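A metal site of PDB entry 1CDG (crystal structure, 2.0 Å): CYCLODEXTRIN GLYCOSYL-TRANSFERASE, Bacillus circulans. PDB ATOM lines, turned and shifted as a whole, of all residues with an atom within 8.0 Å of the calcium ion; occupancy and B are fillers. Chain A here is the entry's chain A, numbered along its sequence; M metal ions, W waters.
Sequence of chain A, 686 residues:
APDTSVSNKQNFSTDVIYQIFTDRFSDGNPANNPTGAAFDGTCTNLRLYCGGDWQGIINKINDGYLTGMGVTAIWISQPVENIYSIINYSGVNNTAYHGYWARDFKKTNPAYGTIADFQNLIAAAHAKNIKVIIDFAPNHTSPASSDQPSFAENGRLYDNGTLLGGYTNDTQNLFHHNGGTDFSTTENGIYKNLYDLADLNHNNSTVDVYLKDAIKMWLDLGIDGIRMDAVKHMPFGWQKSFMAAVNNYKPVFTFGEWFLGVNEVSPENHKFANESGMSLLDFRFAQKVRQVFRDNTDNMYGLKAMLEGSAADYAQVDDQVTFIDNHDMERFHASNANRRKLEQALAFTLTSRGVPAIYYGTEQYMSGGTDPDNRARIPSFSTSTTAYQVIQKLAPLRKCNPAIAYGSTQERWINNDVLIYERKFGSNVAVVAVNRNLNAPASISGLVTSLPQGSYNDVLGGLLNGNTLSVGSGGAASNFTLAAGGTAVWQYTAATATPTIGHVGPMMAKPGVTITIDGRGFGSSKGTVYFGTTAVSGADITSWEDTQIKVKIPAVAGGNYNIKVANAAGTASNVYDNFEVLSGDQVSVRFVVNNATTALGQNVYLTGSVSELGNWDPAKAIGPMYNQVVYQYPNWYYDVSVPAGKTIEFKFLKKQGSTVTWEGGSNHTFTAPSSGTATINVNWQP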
ATOM      1  N   PRO A 138     -21.823   5.798   9.515  1.00  0.00           N
ATOM      2  CA  PRO A 138     -21.196   4.632   8.891  1.00  0.00           C
ATOM      3  C   PRO A 138     -19.699   4.488   9.116  1.00  0.00           C
ATOM      4  O   PRO A 138     -18.984   3.752   8.420  1.00  0.00           O
ATOM      5  CB  PRO A 138     -21.374   4.844   7.394  1.00  0.00           C
ATOM      6  CG  PRO A 138     -21.556   6.336   7.197  1.00  0.00           C
ATOM      7  CD  PRO A 138     -22.090   6.880   8.536  1.00  0.00           C
ATOM      8  N   ASN A 139     -19.182   5.206  10.055  1.00  0.00           N
ATOM      9  CA  ASN A 139     -17.754   5.067  10.179  1.00  0.00           C
ATOM     10  C   ASN A 139     -17.331   3.847  11.030  1.00  0.00           C
ATOM     11  O   ASN A 139     -16.200   3.332  10.895  1.00  0.00           O
ATOM     12  CB  ASN A 139     -17.156   6.356  10.777  1.00  0.00           C
ATOM     13  CG  ASN A 139     -15.719   6.186  11.264  1.00  0.00           C
ATOM     14  OD1 ASN A 139     -14.742   6.149  10.481  1.00  0.00           O
ATOM     15  ND2 ASN A 139     -15.582   6.158  12.571  1.00  0.00           N
ATOM     16  N   HIS A 140     -18.199   3.455  11.928  1.00  0.00           N
ATOM     17  CA  HIS A 140     -17.909   2.431  12.881  1.00  0.00           C
ATOM     18  C   HIS A 140     -19.199   1.820  13.380  1.00  0.00           C
ATOM     19  O   HIS A 140     -20.323   2.295  13.101  1.00  0.00           O
ATOM     20  CB  HIS A 140     -17.280   3.121  14.129  1.00  0.00           C
ATOM     21  CG  HIS A 140     -18.178   4.195  14.705  1.00  0.00           C
ATOM     22  ND1 HIS A 140     -18.021   5.552  14.390  1.00  0.00           N
ATOM     23  CD2 HIS A 140     -19.281   4.104  15.483  1.00  0.00           C
ATOM     24  CE1 HIS A 140     -19.024   6.221  14.962  1.00  0.00           C
ATOM     25  NE2 HIS A 140     -19.787   5.382  15.645  1.00  0.00           N
ATOM     26  N   HIS A 176     -10.932  -2.277  10.729  1.00  0.00           N
ATOM     27  CA  HIS A 176      -9.527  -1.929  10.623  1.00  0.00           C
ATOM     28  C   HIS A 176      -8.874  -2.405  11.905  1.00  0.00           C
ATOM     29  O   HIS A 176      -9.527  -2.380  12.981  1.00  0.00           O
ATOM     30  CB  HIS A 176      -9.268  -0.438  10.520  1.00  0.00           C
ATOM     31  CG  HIS A 176      -9.480   0.129   9.161  1.00  0.00           C
ATOM     32  ND1 HIS A 176     -10.273   1.248   8.972  1.00  0.00           N
ATOM     33  CD2 HIS A 176      -8.948  -0.225   7.968  1.00  0.00           C
ATOM     34  CE1 HIS A 176     -10.218   1.529   7.679  1.00  0.00           C
ATOM     35  NE2 HIS A 176      -9.426   0.666   7.048  1.00  0.00           N
ATOM     36  N   GLU A 187      -4.811  11.300   7.671  1.00  0.00           N
ATOM     37  CA  GLU A 187      -4.673   9.913   7.282  1.00  0.00           C
ATOM     38  C   GLU A 187      -4.799   9.051   8.507  1.00  0.00           C
ATOM     39  O   GLU A 187      -5.401   7.989   8.455  1.00  0.00           O
ATOM     40  CB  GLU A 187      -3.331   9.624   6.572  1.00  0.00           C
ATOM     41  CG  GLU A 187      -3.127   8.129   6.360  1.00  0.00           C
ATOM     42  CD  GLU A 187      -1.806   7.886   5.681  1.00  0.00           C
ATOM     43  OE1 GLU A 187      -1.032   8.814   5.408  1.00  0.00           O
ATOM     44  OE2 GLU A 187      -1.575   6.678   5.398  1.00  0.00           O
ATOM     45  N   ASN A 188      -4.172   9.538   9.581  1.00  0.00           N
ATOM     46  CA  ASN A 188      -4.149   8.897  10.851  1.00  0.00           C
ATOM     47  C   ASN A 188      -5.557   8.731  11.481  1.00  0.00           C
ATOM     48  O   ASN A 188      -5.848   7.630  11.961  1.00  0.00           O
ATOM     49  CB  ASN A 188      -3.131   9.577  11.773  1.00  0.00           C
ATOM     50  CG  ASN A 188      -2.907   8.741  13.025  1.00  0.00           C
ATOM     51  OD1 ASN A 188      -3.765   8.630  13.945  1.00  0.00           O
ATOM     52  ND2 ASN A 188      -1.744   8.149  13.075  1.00  0.00           N
ATOM     53  N   GLY A 189      -6.473   9.759  11.459  1.00  0.00           N
ATOM     54  CA  GLY A 189      -7.859   9.708  12.008  1.00  0.00           C
ATOM     55  C   GLY A 189      -8.911   9.002  11.082  1.00  0.00           C
ATOM     56  O   GLY A 189     -10.044   8.746  11.487  1.00  0.00           O
ATOM     57  N   ILE A 190      -8.468   8.630   9.868  1.00  0.00           N
ATOM     58  CA  ILE A 190      -9.292   7.925   8.890  1.00  0.00           C
ATOM     59  C   ILE A 190      -9.191   6.388   9.014  1.00  0.00           C
ATOM     60  O   ILE A 190     -10.220   5.732   9.159  1.00  0.00           O
ATOM     61  CB  ILE A 190      -9.009   8.321   7.438  1.00  0.00           C
ATOM     62  CG1 ILE A 190      -9.487   9.759   7.166  1.00  0.00           C
ATOM     63  CG2 ILE A 190      -9.813   7.342   6.578  1.00  0.00           C
ATOM     64  CD1 ILE A 190      -8.999  10.268   5.807  1.00  0.00           C
ATOM     65  N   TYR A 191      -7.955   5.873   8.959  1.00  0.00           N
ATOM     66  CA  TYR A 191      -7.573   4.440   8.998  1.00  0.00           C
ATOM     67  C   TYR A 191      -7.292   3.761  10.334  1.00  0.00           C
ATOM     68  O   TYR A 191      -6.896   2.585  10.356  1.00  0.00           O
ATOM     69  CB  TYR A 191      -6.480   4.115   7.961  1.00  0.00           C
ATOM     70  CG  TYR A 191      -6.895   4.530   6.575  1.00  0.00           C
ATOM     71  CD1 TYR A 191      -7.782   3.765   5.805  1.00  0.00           C
ATOM     72  CD2 TYR A 191      -6.455   5.746   6.055  1.00  0.00           C
ATOM     73  CE1 TYR A 191      -8.145   4.119   4.502  1.00  0.00           C
ATOM     74  CE2 TYR A 191      -6.876   6.148   4.788  1.00  0.00           C
ATOM     75  CZ  TYR A 191      -7.686   5.330   4.003  1.00  0.00           C
ATOM     76  OH  TYR A 191      -8.088   5.775   2.748  1.00  0.00           O
ATOM     77  N   LYS A 192      -7.490   4.468  11.437  1.00  0.00           N
ATOM     78  CA  LYS A 192      -7.305   3.896  12.760  1.00  0.00           C
ATOM     79  C   LYS A 192      -8.607   4.118  13.485  1.00  0.00           C
ATOM     80  O   LYS A 192      -9.393   4.924  13.009  1.00  0.00           O
ATOM     81  CB  LYS A 192      -6.130   4.511  13.542  1.00  0.00           C
ATOM     82  CG  LYS A 192      -4.859   4.450  12.759  1.00  0.00           C
ATOM     83  CD  LYS A 192      -3.649   4.537  13.632  1.00  0.00           C
ATOM     84  CE  LYS A 192      -2.414   4.387  12.811  1.00  0.00           C
ATOM     85  NZ  LYS A 192      -1.246   4.682  13.637  1.00  0.00           N
ATOM     86  N   ASN A 193      -8.870   3.444  14.619  1.00  0.00           N
ATOM     87  CA  ASN A 193     -10.112   3.612  15.324  1.00  0.00           C
ATOM     88  C   ASN A 193     -10.255   4.941  16.062  1.00  0.00           C
ATOM     89  O   ASN A 193      -9.280   5.478  16.589  1.00  0.00           O
ATOM     90  CB  ASN A 193     -10.251   2.554  16.415  1.00  0.00           C
ATOM     91  CG  ASN A 193     -10.222   1.122  15.969  1.00  0.00           C
ATOM     92  OD1 ASN A 193     -10.433   0.783  14.816  1.00  0.00           O
ATOM     93  ND2 ASN A 193     -10.016   0.244  16.927  1.00  0.00           N
ATOM     94  N   LEU A 194     -11.480   5.428  16.199  1.00  0.00           N
ATOM     95  CA  LEU A 194     -11.678   6.604  17.007  1.00  0.00           C
ATOM     96  C   LEU A 194     -11.889   6.138  18.446  1.00  0.00           C
ATOM     97  O   LEU A 194     -12.919   5.549  18.675  1.00  0.00           O
ATOM     98  CB  LEU A 194     -12.981   7.304  16.606  1.00  0.00           C
ATOM     99  CG  LEU A 194     -12.840   8.103  15.352  1.00  0.00           C
ATOM    100  CD1 LEU A 194     -14.145   8.835  15.116  1.00  0.00           C
ATOM    101  CD2 LEU A 194     -11.695   9.090  15.485  1.00  0.00           C
ATOM    102  N   LEU A 197     -13.930   2.630  19.171  1.00  0.00           N
ATOM    103  CA  LEU A 197     -15.036   2.268  18.321  1.00  0.00           C
ATOM    104  C   LEU A 197     -14.509   1.391  17.237  1.00  0.00           C
ATOM    105  O   LEU A 197     -13.527   1.765  16.639  1.00  0.00           O
ATOM    106  CB  LEU A 197     -15.661   3.527  17.692  1.00  0.00           C
ATOM    107  CG  LEU A 197     -16.472   4.334  18.706  1.00  0.00           C
ATOM    108  CD1 LEU A 197     -16.736   5.772  18.230  1.00  0.00           C
ATOM    109  CD2 LEU A 197     -17.759   3.634  19.094  1.00  0.00           C
ATOM    110  N   ALA A 198     -15.156   0.265  16.947  1.00  0.00           N
ATOM    111  CA  ALA A 198     -14.689  -0.628  15.865  1.00  0.00           C
ATOM    112  C   ALA A 198     -14.833   0.054  14.482  1.00  0.00           C
ATOM    113  O   ALA A 198     -15.940   0.425  14.055  1.00  0.00           O
ATOM    114  CB  ALA A 198     -15.565  -1.838  15.900  1.00  0.00           C
ATOM    115  N   ASP A 199     -13.693   0.288  13.823  1.00  0.00           N
ATOM    116  CA  ASP A 199     -13.671   1.039  12.598  1.00  0.00           C
ATOM    117  C   ASP A 199     -13.942   0.207  11.386  1.00  0.00           C
ATOM    118  O   ASP A 199     -13.152  -0.686  11.070  1.00  0.00           O
ATOM    119  CB  ASP A 199     -12.347   1.792  12.432  1.00  0.00           C
ATOM    120  CG  ASP A 199     -12.410   3.100  11.653  1.00  0.00           C
ATOM    121  OD1 ASP A 199     -13.199   4.024  11.986  1.00  0.00           O
ATOM    122  OD2 ASP A 199     -11.633   3.158  10.640  1.00  0.00           O
ATOM    123  N   LEU A 200     -15.024   0.560  10.680  1.00  0.00           N
ATOM    124  CA  LEU A 200     -15.414  -0.161   9.478  1.00  0.00           C
ATOM    125  C   LEU A 200     -14.383  -0.005   8.344  1.00  0.00           C
ATOM    126  O   LEU A 200     -13.869   1.090   8.019  1.00  0.00           O
ATOM    127  CB  LEU A 200     -16.871   0.208   9.019  1.00  0.00           C
ATOM    128  CG  LEU A 200     -18.005  -0.264   9.964  1.00  0.00           C
ATOM    129  CD1 LEU A 200     -19.335   0.417   9.671  1.00  0.00           C
ATOM    130  CD2 LEU A 200     -18.214  -1.779   9.900  1.00  0.00           C
ATOM    131  N   ASN A 201     -14.102  -1.110   7.642  1.00  0.00           N
ATOM    132  CA  ASN A 201     -13.207  -1.034   6.515  1.00  0.00           C
ATOM    133  C   ASN A 201     -14.011  -0.834   5.256  1.00  0.00           C
ATOM    134  O   ASN A 201     -14.490  -1.809   4.666  1.00  0.00           O
ATOM    135  CB  ASN A 201     -12.388  -2.318   6.436  1.00  0.00           C
ATOM    136  CG  ASN A 201     -11.576  -2.390   5.165  1.00  0.00           C
ATOM    137  OD1 ASN A 201     -11.413  -1.372   4.450  1.00  0.00           O
ATOM    138  ND2 ASN A 201     -11.074  -3.574   4.845  1.00  0.00           N
ATOM    139  N   HIS A 202     -14.176   0.402   4.766  1.00  0.00           N
ATOM    140  CA  HIS A 202     -14.994   0.587   3.565  1.00  0.00           C
ATOM    141  C   HIS A 202     -14.400   0.042   2.316  1.00  0.00           C
ATOM    142  O   HIS A 202     -15.050   0.057   1.270  1.00  0.00           O
ATOM    143  CB  HIS A 202     -15.527   2.022   3.323  1.00  0.00           C
ATOM    144  CG  HIS A 202     -16.194   2.525   4.559  1.00  0.00           C
ATOM    145  ND1 HIS A 202     -15.468   3.143   5.556  1.00  0.00           N
ATOM    146  CD2 HIS A 202     -17.487   2.472   4.955  1.00  0.00           C
ATOM    147  CE1 HIS A 202     -16.345   3.436   6.543  1.00  0.00           C
ATOM    148  NE2 HIS A 202     -17.555   3.047   6.218  1.00  0.00           N
ATOM    149  N   ALA A 230     -18.893  11.922  11.527  1.00  0.00           N
ATOM    150  CA  ALA A 230     -17.432  11.697  11.415  1.00  0.00           C
ATOM    151  C   ALA A 230     -16.875  11.670  10.017  1.00  0.00           C
ATOM    152  O   ALA A 230     -16.048  10.840   9.663  1.00  0.00           O
ATOM    153  CB  ALA A 230     -17.065  10.392  12.102  1.00  0.00           C
ATOM    154  N   LYS A 232     -14.736  13.449   8.661  1.00  0.00           N
ATOM    155  CA  LYS A 232     -13.287  13.594   8.505  1.00  0.00           C
ATOM    156  C   LYS A 232     -12.500  12.259   8.812  1.00  0.00           C
ATOM    157  O   LYS A 232     -11.242  12.215   8.608  1.00  0.00           O
ATOM    158  CB  LYS A 232     -12.871  14.620   9.544  1.00  0.00           C
ATOM    159  CG  LYS A 232     -11.480  15.132   9.356  1.00  0.00           C
ATOM    160  CD  LYS A 232     -11.075  15.777  10.671  1.00  0.00           C
ATOM    161  CE  LYS A 232     -10.027  16.890  10.631  1.00  0.00           C
ATOM    162  NZ  LYS A 232      -8.639  16.446  10.367  1.00  0.00           N
ATOM    163  N   HIS A 233     -13.242  11.206   9.277  1.00  0.00           N
ATOM    164  CA  HIS A 233     -12.717   9.880   9.699  1.00  0.00           C
ATOM    165  C   HIS A 233     -12.963   8.679   8.764  1.00  0.00           C
ATOM    166  O   HIS A 233     -12.619   7.520   9.080  1.00  0.00           O
ATOM    167  CB  HIS A 233     -13.149   9.566  11.142  1.00  0.00           C
ATOM    168  CG  HIS A 233     -12.705  10.708  11.991  1.00  0.00           C
ATOM    169  ND1 HIS A 233     -11.374  10.888  12.310  1.00  0.00           N
ATOM    170  CD2 HIS A 233     -13.389  11.797  12.472  1.00  0.00           C
ATOM    171  CE1 HIS A 233     -11.292  12.031  13.011  1.00  0.00           C
ATOM    172  NE2 HIS A 233     -12.484  12.608  13.120  1.00  0.00           N
ATOM    173  N   MET A 234     -13.494   8.974   7.589  1.00  0.00           N
ATOM    174  CA  MET A 234     -13.764   8.002   6.557  1.00  0.00           C
ATOM    175  C   MET A 234     -13.121   8.491   5.265  1.00  0.00           C
ATOM    176  O   MET A 234     -13.047   9.702   5.057  1.00  0.00           O
ATOM    177  CB  MET A 234     -15.290   7.930   6.355  1.00  0.00           C
ATOM    178  CG  MET A 234     -16.004   7.235   7.456  1.00  0.00           C
ATOM    179  SD  MET A 234     -17.774   7.183   7.178  1.00  0.00           S
ATOM    180  CE  MET A 234     -18.162   8.947   7.333  1.00  0.00           C
ATOM    181  N   PRO A 235     -12.754   7.556   4.372  1.00  0.00           N
ATOM    182  CA  PRO A 235     -12.134   7.916   3.118  1.00  0.00           C
ATOM    183  C   PRO A 235     -12.974   8.893   2.295  1.00  0.00           C
ATOM    184  O   PRO A 235     -14.182   8.684   2.080  1.00  0.00           O
ATOM    185  CB  PRO A 235     -11.894   6.610   2.394  1.00  0.00           C
ATOM    186  CG  PRO A 235     -12.014   5.478   3.421  1.00  0.00           C
ATOM    187  CD  PRO A 235     -12.751   6.062   4.596  1.00  0.00           C
HETATM  188 CA    CA M   1     -12.638   5.349   9.983  1.00  0.00          CA
HETATM  189  O   HOH W   1     -12.067   4.859   7.749  1.00  0.00           O
HETATM  190  O   HOH W   2     -14.264   3.858   9.232  1.00  0.00           O
HETATM  191  O   HOH W   3     -11.457   6.707  11.855  1.00  0.00           O
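The calcium ion is bound by OD1 of Asn 139, water W2, O of His 233, water W1, OD1 of Asp 199, OD2 of Asp 199, O of Ile 190 and water W3.
The calcium ion has eight donor atoms within binding distance.
Water W2 lies within hydrogen-bond range of O of Asn 139 and O of Leu 200.
The backbone NH of Leu 200 sits at hydrogen-bond distance from the backbone carbonyl oxygen of Asn 139.
The backbone NH (N) of His 176 is in hydrogen-bond range of the backbone carbonyl oxygen (O) of Asp 199.
The side-chain amide nitrogen (ND2) of Asn 139 is in hydrogen-bond range of a ring nitrogen (ND1) of His 140 (3.1 Å).
The backbone NH (N) of Asn 139 lies close to the side-chain sulfur (SD) of Met 234, 3.8 Å away.
ND1 of His 233 lies within hydrogen-bond range of O of Gly 189.
The backbone NH of Asp 199 sits close to the side-chain amide oxygen of Asn 193, 3.4 Å away.
Within 4 Å of the calcium ion: Asn 139, Ile 190, Asp 199 and His 233.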
